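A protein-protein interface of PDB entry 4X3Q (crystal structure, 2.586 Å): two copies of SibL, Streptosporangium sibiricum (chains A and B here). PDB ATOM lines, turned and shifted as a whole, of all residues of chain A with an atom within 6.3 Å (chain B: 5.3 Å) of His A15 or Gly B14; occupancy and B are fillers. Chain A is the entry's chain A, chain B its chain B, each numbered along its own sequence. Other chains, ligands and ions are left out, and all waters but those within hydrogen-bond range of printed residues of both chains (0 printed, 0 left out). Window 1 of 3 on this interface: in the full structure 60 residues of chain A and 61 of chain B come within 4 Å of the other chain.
The backbone carbonyl oxygen (O) of Leu A12 sits at hydrogen-bond distance from the side-chain amide nitrogen (NE2) of Gln B100, 3.1 Å away. N of His A15 lies within hydrogen-bond range of O of Gly B14 (3.5 Å). The side-chain hydroxyl (OH) of Tyr A105 sits at hydrogen-bond distance from the backbone carbonyl oxygen (O) of Tyr B105 (2.7 Å). O of Gly B14 sits close to O of Gly A14 (3.4 Å).
The backbone carbonyl oxygen (O) of Gln B100 lies within hydrogen-bond range of the backbone NH (N) of Tyr B105 (2.7 Å).
Phe B18 touches Val A11. His A15 touches His B15 (CA to CA, 3.6 Å). Gln B100 touches His A15. CE1 of Tyr B105 touches CB of His A15 (3.6 Å). Val B11 touches Phe A18 (O to CA, 3.4 Å). Leu B12 touches Phe A18. O of Ala B108 touches CD of Gln A19, 3.4 Å away. His B15 touches Tyr A105. Ala B16 touches Leu A291. CA of Ala B17 touches CD2 of Leu A291, at 3.8 Å.
His A15 touches just these residues of chain B: Gly B14 (3.5 Å), His B15 (3.6 Å), Gln B100 (3.7 Å), Tyr B105 (3.6 Å) and Ala B108 (3.6 Å). Gly B14 touches two residues of chain A. Of the printed residues of chain A, Phe B18 touches Val A11 and Leu A12. Of the printed residues of chain B, Leu A12 touches Phe B18 and Gln B100. Ala B104 touches none of the printed residues of chain A. The nearest residue of chain A that does not touch Gly B14 is Phe A18 (4.3 Å). The nearest printed residue of chain A that does not touch Ala B16 is His A15 (5.9 Å).
Along chain B the printed residues that touch a printed residue of chain A span positions 11 to 108. Among the printed residues, 23 pairs touch across the chains. Among the printed residues, no Asp or Glu carboxylate lies within 4 Å of a Lys or Arg side-chain nitrogen of the other chain.
Gly B14 touches its own counterpart, Gly A14. His B15 touches its own counterpart, His A15. His A15 touches Tyr B105, and with the chains exchanged Tyr A105 touches His B15. Phe A18 touches His B15, but with the chains exchanged His A15 does not touch Phe B18 (4.1 Å). 10 positions are printed for both chains. Of the 23 pairs that touch across the chains among the printed residues, 13 have their exchanged pair printed and touching as well.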
ATOM      1  N   PRO A  10       2.414  18.728  -2.589  1.00  0.00           N
ATOM      2  CA  PRO A  10       3.425  17.705  -2.895  1.00  0.00           C
ATOM      3  C   PRO A  10       4.101  17.059  -1.654  1.00  0.00           C
ATOM      4  O   PRO A  10       4.560  15.929  -1.781  1.00  0.00           O
ATOM      5  CB  PRO A  10       4.448  18.470  -3.752  1.00  0.00           C
ATOM      6  CG  PRO A  10       4.208  19.898  -3.475  1.00  0.00           C
ATOM      7  CD  PRO A  10       2.772  20.047  -3.129  1.00  0.00           C
ATOM      8  N   VAL A  11       4.154  17.726  -0.498  1.00  0.00           N
ATOM      9  CA  VAL A  11       4.708  17.084   0.695  1.00  0.00           C
ATOM     10  C   VAL A  11       3.678  16.142   1.285  1.00  0.00           C
ATOM     11  O   VAL A  11       3.969  14.978   1.597  1.00  0.00           O
ATOM     12  CB  VAL A  11       5.158  18.101   1.772  1.00  0.00           C
ATOM     13  CG1 VAL A  11       5.688  17.390   3.017  1.00  0.00           C
ATOM     14  CG2 VAL A  11       6.198  19.050   1.211  1.00  0.00           C
ATOM     15  N   LEU A  12       2.464  16.655   1.417  1.00  0.00           N
ATOM     16  CA  LEU A  12       1.333  15.890   1.940  1.00  0.00           C
ATOM     17  C   LEU A  12       1.088  14.600   1.128  1.00  0.00           C
ATOM     18  O   LEU A  12       0.547  13.621   1.637  1.00  0.00           O
ATOM     19  CB  LEU A  12       0.081  16.774   1.937  1.00  0.00           C
ATOM     20  CG  LEU A  12      -1.242  16.217   2.445  1.00  0.00           C
ATOM     21  CD1 LEU A  12      -1.188  16.006   3.950  1.00  0.00           C
ATOM     22  CD2 LEU A  12      -2.373  17.129   2.033  1.00  0.00           C
ATOM     23  N   PHE A  13       1.461  14.622  -0.146  1.00  0.00           N
ATOM     24  CA  PHE A  13       1.354  13.448  -0.997  1.00  0.00           C
ATOM     25  C   PHE A  13       2.710  12.939  -1.514  1.00  0.00           C
ATOM     26  O   PHE A  13       2.773  12.281  -2.564  1.00  0.00           O
ATOM     27  CB  PHE A  13       0.438  13.736  -2.183  1.00  0.00           C
ATOM     28  CG  PHE A  13      -0.996  13.898  -1.815  1.00  0.00           C
ATOM     29  CD1 PHE A  13      -1.849  12.816  -1.849  1.00  0.00           C
ATOM     30  CD2 PHE A  13      -1.499  15.124  -1.445  1.00  0.00           C
ATOM     31  CE1 PHE A  13      -3.178  12.948  -1.519  1.00  0.00           C
ATOM     32  CE2 PHE A  13      -2.833  15.265  -1.117  1.00  0.00           C
ATOM     33  CZ  PHE A  13      -3.672  14.170  -1.152  1.00  0.00           C
ATOM     34  N   GLY A  14       3.780  13.237  -0.777  1.00  0.00           N
ATOM     35  CA  GLY A  14       5.121  12.887  -1.210  1.00  0.00           C
ATOM     36  C   GLY A  14       5.352  11.406  -1.448  1.00  0.00           C
ATOM     37  O   GLY A  14       6.046  11.013  -2.378  1.00  0.00           O
ATOM     38  N   HIS A  15       4.811  10.582  -0.564  1.00  0.00           N
ATOM     39  CA  HIS A  15       4.973   9.141  -0.664  1.00  0.00           C
ATOM     40  C   HIS A  15       4.298   8.655  -1.924  1.00  0.00           C
ATOM     41  O   HIS A  15       4.763   7.717  -2.560  1.00  0.00           O
ATOM     42  CB  HIS A  15       4.385   8.448   0.567  1.00  0.00           C
ATOM     43  CG  HIS A  15       2.911   8.645   0.707  1.00  0.00           C
ATOM     44  ND1 HIS A  15       2.354   9.862   1.044  1.00  0.00           N
ATOM     45  CD2 HIS A  15       1.877   7.783   0.554  1.00  0.00           C
ATOM     46  CE1 HIS A  15       1.039   9.740   1.087  1.00  0.00           C
ATOM     47  NE2 HIS A  15       0.725   8.488   0.793  1.00  0.00           N
ATOM     48  N   ALA A  16       3.195   9.313  -2.278  1.00  0.00           N
ATOM     49  CA  ALA A  16       2.454   8.971  -3.479  1.00  0.00           C
ATOM     50  C   ALA A  16       3.263   9.377  -4.715  1.00  0.00           C
ATOM     51  O   ALA A  16       3.245   8.700  -5.749  1.00  0.00           O
ATOM     52  CB  ALA A  16       1.106   9.659  -3.471  1.00  0.00           C
ATOM     53  N   ALA A  17       3.968  10.497  -4.593  1.00  0.00           N
ATOM     54  CA  ALA A  17       4.848  10.976  -5.646  1.00  0.00           C
ATOM     55  C   ALA A  17       5.934   9.941  -5.896  1.00  0.00           C
ATOM     56  O   ALA A  17       6.227   9.597  -7.048  1.00  0.00           O
ATOM     57  CB  ALA A  17       5.458  12.322  -5.270  1.00  0.00           C
ATOM     58  N   PHE A  18       6.533   9.451  -4.812  1.00  0.00           N
ATOM     59  CA  PHE A  18       7.547   8.421  -4.934  1.00  0.00           C
ATOM     60  C   PHE A  18       6.996   7.166  -5.620  1.00  0.00           C
ATOM     61  O   PHE A  18       7.674   6.542  -6.450  1.00  0.00           O
ATOM     62  CB  PHE A  18       8.120   8.030  -3.578  1.00  0.00           C
ATOM     63  CG  PHE A  18       8.894   6.756  -3.629  1.00  0.00           C
ATOM     64  CD1 PHE A  18      10.165   6.730  -4.210  1.00  0.00           C
ATOM     65  CD2 PHE A  18       8.338   5.565  -3.169  1.00  0.00           C
ATOM     66  CE1 PHE A  18      10.885   5.539  -4.305  1.00  0.00           C
ATOM     67  CE2 PHE A  18       9.054   4.368  -3.261  1.00  0.00           C
ATOM     68  CZ  PHE A  18      10.326   4.356  -3.833  1.00  0.00           C
ATOM     69  N   GLN A  19       5.776   6.785  -5.254  1.00  0.00           N
ATOM     70  CA  GLN A  19       5.186   5.551  -5.769  1.00  0.00           C
ATOM     71  C   GLN A  19       4.997   5.592  -7.282  1.00  0.00           C
ATOM     72  O   GLN A  19       5.038   4.552  -7.936  1.00  0.00           O
ATOM     73  CB  GLN A  19       3.855   5.251  -5.066  1.00  0.00           C
ATOM     74  CG  GLN A  19       4.031   4.774  -3.639  1.00  0.00           C
ATOM     75  CD  GLN A  19       4.917   3.523  -3.509  1.00  0.00           C
ATOM     76  OE1 GLN A  19       5.017   2.696  -4.435  1.00  0.00           O
ATOM     77  NE2 GLN A  19       5.571   3.389  -2.354  1.00  0.00           N
ATOM     78  N   GLN A  20       4.776   6.782  -7.831  1.00  0.00           N
ATOM     79  CA  GLN A  20       4.664   6.940  -9.277  1.00  0.00           C
ATOM     80  C   GLN A  20       5.995   6.621  -9.989  1.00  0.00           C
ATOM     81  O   GLN A  20       6.033   5.899 -11.006  1.00  0.00           O
ATOM     82  CB  GLN A  20       4.224   8.365  -9.620  1.00  0.00           C
ATOM     83  CG  GLN A  20       2.872   8.775  -9.025  1.00  0.00           C
ATOM     84  CD  GLN A  20       1.699   8.041  -9.627  1.00  0.00           C
ATOM     85  OE1 GLN A  20       1.854   7.139 -10.441  1.00  0.00           O
ATOM     86  NE2 GLN A  20       0.505   8.413  -9.202  1.00  0.00           N
ATOM     87  N   TYR A 105      11.409   2.539   2.169  1.00  0.00           N
ATOM     88  CA  TYR A 105      10.052   3.058   2.234  1.00  0.00           C
ATOM     89  C   TYR A 105       9.308   2.668   3.503  1.00  0.00           C
ATOM     90  O   TYR A 105       8.776   3.532   4.220  1.00  0.00           O
ATOM     91  CB  TYR A 105       9.246   2.579   1.021  1.00  0.00           C
ATOM     92  CG  TYR A 105       7.868   3.186   0.978  1.00  0.00           C
ATOM     93  CD1 TYR A 105       7.615   4.320   0.224  1.00  0.00           C
ATOM     94  CD2 TYR A 105       6.820   2.638   1.716  1.00  0.00           C
ATOM     95  CE1 TYR A 105       6.360   4.887   0.202  1.00  0.00           C
ATOM     96  CE2 TYR A 105       5.569   3.194   1.694  1.00  0.00           C
ATOM     97  CZ  TYR A 105       5.339   4.316   0.936  1.00  0.00           C
ATOM     98  OH  TYR A 105       4.085   4.862   0.915  1.00  0.00           O
ATOM     99  N   LEU A 291      16.245  15.175   3.476  1.00  0.00           N
ATOM    100  CA  LEU A 291      15.299  14.102   3.255  1.00  0.00           C
ATOM    101  C   LEU A 291      15.894  12.733   3.519  1.00  0.00           C
ATOM    102  O   LEU A 291      15.258  11.891   4.141  1.00  0.00           O
ATOM    103  CB  LEU A 291      14.713  14.195   1.845  1.00  0.00           C
ATOM    104  CG  LEU A 291      13.898  15.490   1.654  1.00  0.00           C
ATOM    105  CD1 LEU A 291      13.116  15.458   0.364  1.00  0.00           C
ATOM    106  CD2 LEU A 291      12.970  15.771   2.854  1.00  0.00           C
ATOM    107  N   VAL B   9      14.974  14.525  -7.150  1.00  0.00           N
ATOM    108  CA  VAL B   9      15.255  14.378  -5.726  1.00  0.00           C
ATOM    109  C   VAL B   9      13.980  14.425  -4.884  1.00  0.00           C
ATOM    110  O   VAL B   9      13.734  13.487  -4.119  1.00  0.00           O
ATOM    111  CB  VAL B   9      16.279  15.448  -5.236  1.00  0.00           C
ATOM    112  CG1 VAL B   9      16.337  15.514  -3.728  1.00  0.00           C
ATOM    113  CG2 VAL B   9      17.662  15.134  -5.776  1.00  0.00           C
ATOM    114  N   PRO B  10      13.132  15.470  -5.050  1.00  0.00           N
ATOM    115  CA  PRO B  10      11.928  15.464  -4.196  1.00  0.00           C
ATOM    116  C   PRO B  10      10.989  14.302  -4.468  1.00  0.00           C
ATOM    117  O   PRO B  10      10.201  13.981  -3.594  1.00  0.00           O
ATOM    118  CB  PRO B  10      11.232  16.794  -4.530  1.00  0.00           C
ATOM    119  CG  PRO B  10      11.804  17.241  -5.821  1.00  0.00           C
ATOM    120  CD  PRO B  10      13.206  16.682  -5.891  1.00  0.00           C
ATOM    121  N   VAL B  11      11.037  13.714  -5.657  1.00  0.00           N
ATOM    122  CA  VAL B  11      10.225  12.533  -5.941  1.00  0.00           C
ATOM    123  C   VAL B  11      10.844  11.277  -5.347  1.00  0.00           C
ATOM    124  O   VAL B  11      10.176  10.499  -4.665  1.00  0.00           O
ATOM    125  CB  VAL B  11      10.032  12.324  -7.455  1.00  0.00           C
ATOM    126  CG1 VAL B  11       9.151  11.109  -7.717  1.00  0.00           C
ATOM    127  CG2 VAL B  11       9.437  13.587  -8.095  1.00  0.00           C
ATOM    128  N   LEU B  12      12.137  11.111  -5.611  1.00  0.00           N
ATOM    129  CA  LEU B  12      12.926   9.978  -5.130  1.00  0.00           C
ATOM    130  C   LEU B  12      12.908   9.839  -3.619  1.00  0.00           C
ATOM    131  O   LEU B  12      12.951   8.723  -3.084  1.00  0.00           O
ATOM    132  CB  LEU B  12      14.370  10.119  -5.610  1.00  0.00           C
ATOM    133  CG  LEU B  12      15.328   9.014  -5.185  1.00  0.00           C
ATOM    134  CD1 LEU B  12      14.929   7.697  -5.843  1.00  0.00           C
ATOM    135  CD2 LEU B  12      16.760   9.394  -5.555  1.00  0.00           C
ATOM    136  N   PHE B  13      12.783  10.976  -2.939  1.00  0.00           N
ATOM    137  CA  PHE B  13      12.718  10.997  -1.489  1.00  0.00           C
ATOM    138  C   PHE B  13      11.345  11.504  -1.054  1.00  0.00           C
ATOM    139  O   PHE B  13      11.179  12.017   0.064  1.00  0.00           O
ATOM    140  CB  PHE B  13      13.839  11.874  -0.914  1.00  0.00           C
ATOM    141  CG  PHE B  13      15.220  11.350  -1.189  1.00  0.00           C
ATOM    142  CD1 PHE B  13      15.772  10.354  -0.402  1.00  0.00           C
ATOM    143  CD2 PHE B  13      15.960  11.840  -2.259  1.00  0.00           C
ATOM    144  CE1 PHE B  13      17.046   9.863  -0.663  1.00  0.00           C
ATOM    145  CE2 PHE B  13      17.234  11.362  -2.526  1.00  0.00           C
ATOM    146  CZ  PHE B  13      17.781  10.374  -1.729  1.00  0.00           C
ATOM    147  N   GLY B  14      10.363  11.321  -1.938  1.00  0.00           N
ATOM    148  CA  GLY B  14       9.022  11.843  -1.726  1.00  0.00           C
ATOM    149  C   GLY B  14       8.412  11.369  -0.429  1.00  0.00           C
ATOM    150  O   GLY B  14       7.789  12.146   0.288  1.00  0.00           O
ATOM    151  N   HIS B  15       8.604  10.090  -0.121  1.00  0.00           N
ATOM    152  CA  HIS B  15       8.083   9.522   1.107  1.00  0.00           C
ATOM    153  C   HIS B  15       8.725  10.160   2.352  1.00  0.00           C
ATOM    154  O   HIS B  15       8.074  10.306   3.396  1.00  0.00           O
ATOM    155  CB  HIS B  15       8.281   8.004   1.114  1.00  0.00           C
ATOM    156  CG  HIS B  15       9.712   7.592   1.050  1.00  0.00           C
ATOM    157  ND1 HIS B  15      10.450   7.647  -0.113  1.00  0.00           N
ATOM    158  CD2 HIS B  15      10.567   7.195   2.022  1.00  0.00           C
ATOM    159  CE1 HIS B  15      11.685   7.246   0.134  1.00  0.00           C
ATOM    160  NE2 HIS B  15      11.783   6.970   1.422  1.00  0.00           N
ATOM    161  N   ALA B  16       9.997  10.534   2.234  1.00  0.00           N
ATOM    162  CA  ALA B  16      10.711  11.158   3.346  1.00  0.00           C
ATOM    163  C   ALA B  16      10.208  12.579   3.590  1.00  0.00           C
ATOM    164  O   ALA B  16      10.085  13.019   4.734  1.00  0.00           O
ATOM    165  CB  ALA B  16      12.194  11.169   3.082  1.00  0.00           C
ATOM    166  N   ALA B  17       9.874  13.284   2.515  1.00  0.00           N
ATOM    167  CA  ALA B  17       9.327  14.619   2.653  1.00  0.00           C
ATOM    168  C   ALA B  17       8.046  14.556   3.475  1.00  0.00           C
ATOM    169  O   ALA B  17       7.910  15.286   4.455  1.00  0.00           O
ATOM    170  CB  ALA B  17       9.070  15.239   1.279  1.00  0.00           C
ATOM    171  N   PHE B  18       7.147  13.631   3.125  1.00  0.00           N
ATOM    172  CA  PHE B  18       5.906  13.478   3.867  1.00  0.00           C
ATOM    173  C   PHE B  18       6.198  13.191   5.337  1.00  0.00           C
ATOM    174  O   PHE B  18       5.524  13.754   6.233  1.00  0.00           O
ATOM    175  CB  PHE B  18       5.014  12.360   3.292  1.00  0.00           C
ATOM    176  CG  PHE B  18       3.937  11.921   4.254  1.00  0.00           C
ATOM    177  CD1 PHE B  18       2.813  12.715   4.483  1.00  0.00           C
ATOM    178  CD2 PHE B  18       4.097  10.759   5.015  1.00  0.00           C
ATOM    179  CE1 PHE B  18       1.840  12.334   5.424  1.00  0.00           C
ATOM    180  CE2 PHE B  18       3.127  10.371   5.947  1.00  0.00           C
ATOM    181  CZ  PHE B  18       2.002  11.162   6.154  1.00  0.00           C
ATOM    182  N   GLN B 100      -3.187  10.321   6.447  1.00  0.00           N
ATOM    183  CA  GLN B 100      -2.134   9.837   5.564  1.00  0.00           C
ATOM    184  C   GLN B 100      -1.236   8.825   6.263  1.00  0.00           C
ATOM    185  O   GLN B 100      -0.963   7.748   5.738  1.00  0.00           O
ATOM    186  CB  GLN B 100      -1.276  11.001   5.076  1.00  0.00           C
ATOM    187  CG  GLN B 100      -1.976  12.015   4.209  1.00  0.00           C
ATOM    188  CD  GLN B 100      -2.516  11.410   2.920  1.00  0.00           C
ATOM    189  OE1 GLN B 100      -3.447  10.606   2.942  1.00  0.00           O
ATOM    190  NE2 GLN B 100      -1.935  11.794   1.795  1.00  0.00           N
ATOM    191  N   ALA B 104      -3.098   5.911   4.685  1.00  0.00           N
ATOM    192  CA  ALA B 104      -2.617   5.934   3.299  1.00  0.00           C
ATOM    193  C   ALA B 104      -1.184   5.394   3.119  1.00  0.00           C
ATOM    194  O   ALA B 104      -0.928   4.615   2.208  1.00  0.00           O
ATOM    195  CB  ALA B 104      -2.702   7.352   2.737  1.00  0.00           C
ATOM    196  N   TYR B 105      -0.273   5.779   4.005  1.00  0.00           N
ATOM    197  CA  TYR B 105       1.146   5.605   3.751  1.00  0.00           C
ATOM    198  C   TYR B 105       1.551   4.139   3.487  1.00  0.00           C
ATOM    199  O   TYR B 105       2.203   3.844   2.479  1.00  0.00           O
ATOM    200  CB  TYR B 105       1.988   6.172   4.911  1.00  0.00           C
ATOM    201  CG  TYR B 105       3.469   6.111   4.612  1.00  0.00           C
ATOM    202  CD1 TYR B 105       4.121   7.189   4.036  1.00  0.00           C
ATOM    203  CD2 TYR B 105       4.203   4.948   4.852  1.00  0.00           C
ATOM    204  CE1 TYR B 105       5.465   7.126   3.736  1.00  0.00           C
ATOM    205  CE2 TYR B 105       5.539   4.872   4.546  1.00  0.00           C
ATOM    206  CZ  TYR B 105       6.169   5.964   3.993  1.00  0.00           C
ATOM    207  OH  TYR B 105       7.504   5.896   3.698  1.00  0.00           O
ATOM    208  N   ALA B 108       0.162   2.408   0.401  1.00  0.00           N
ATOM    209  CA  ALA B 108       0.723   3.002  -0.810  1.00  0.00           C
ATOM    210  C   ALA B 108       1.845   2.112  -1.423  1.00  0.00           C
ATOM    211  O   ALA B 108       2.022   2.056  -2.642  1.00  0.00           O
ATOM    212  CB  ALA B 108       1.238   4.424  -0.504  1.00  0.00           C
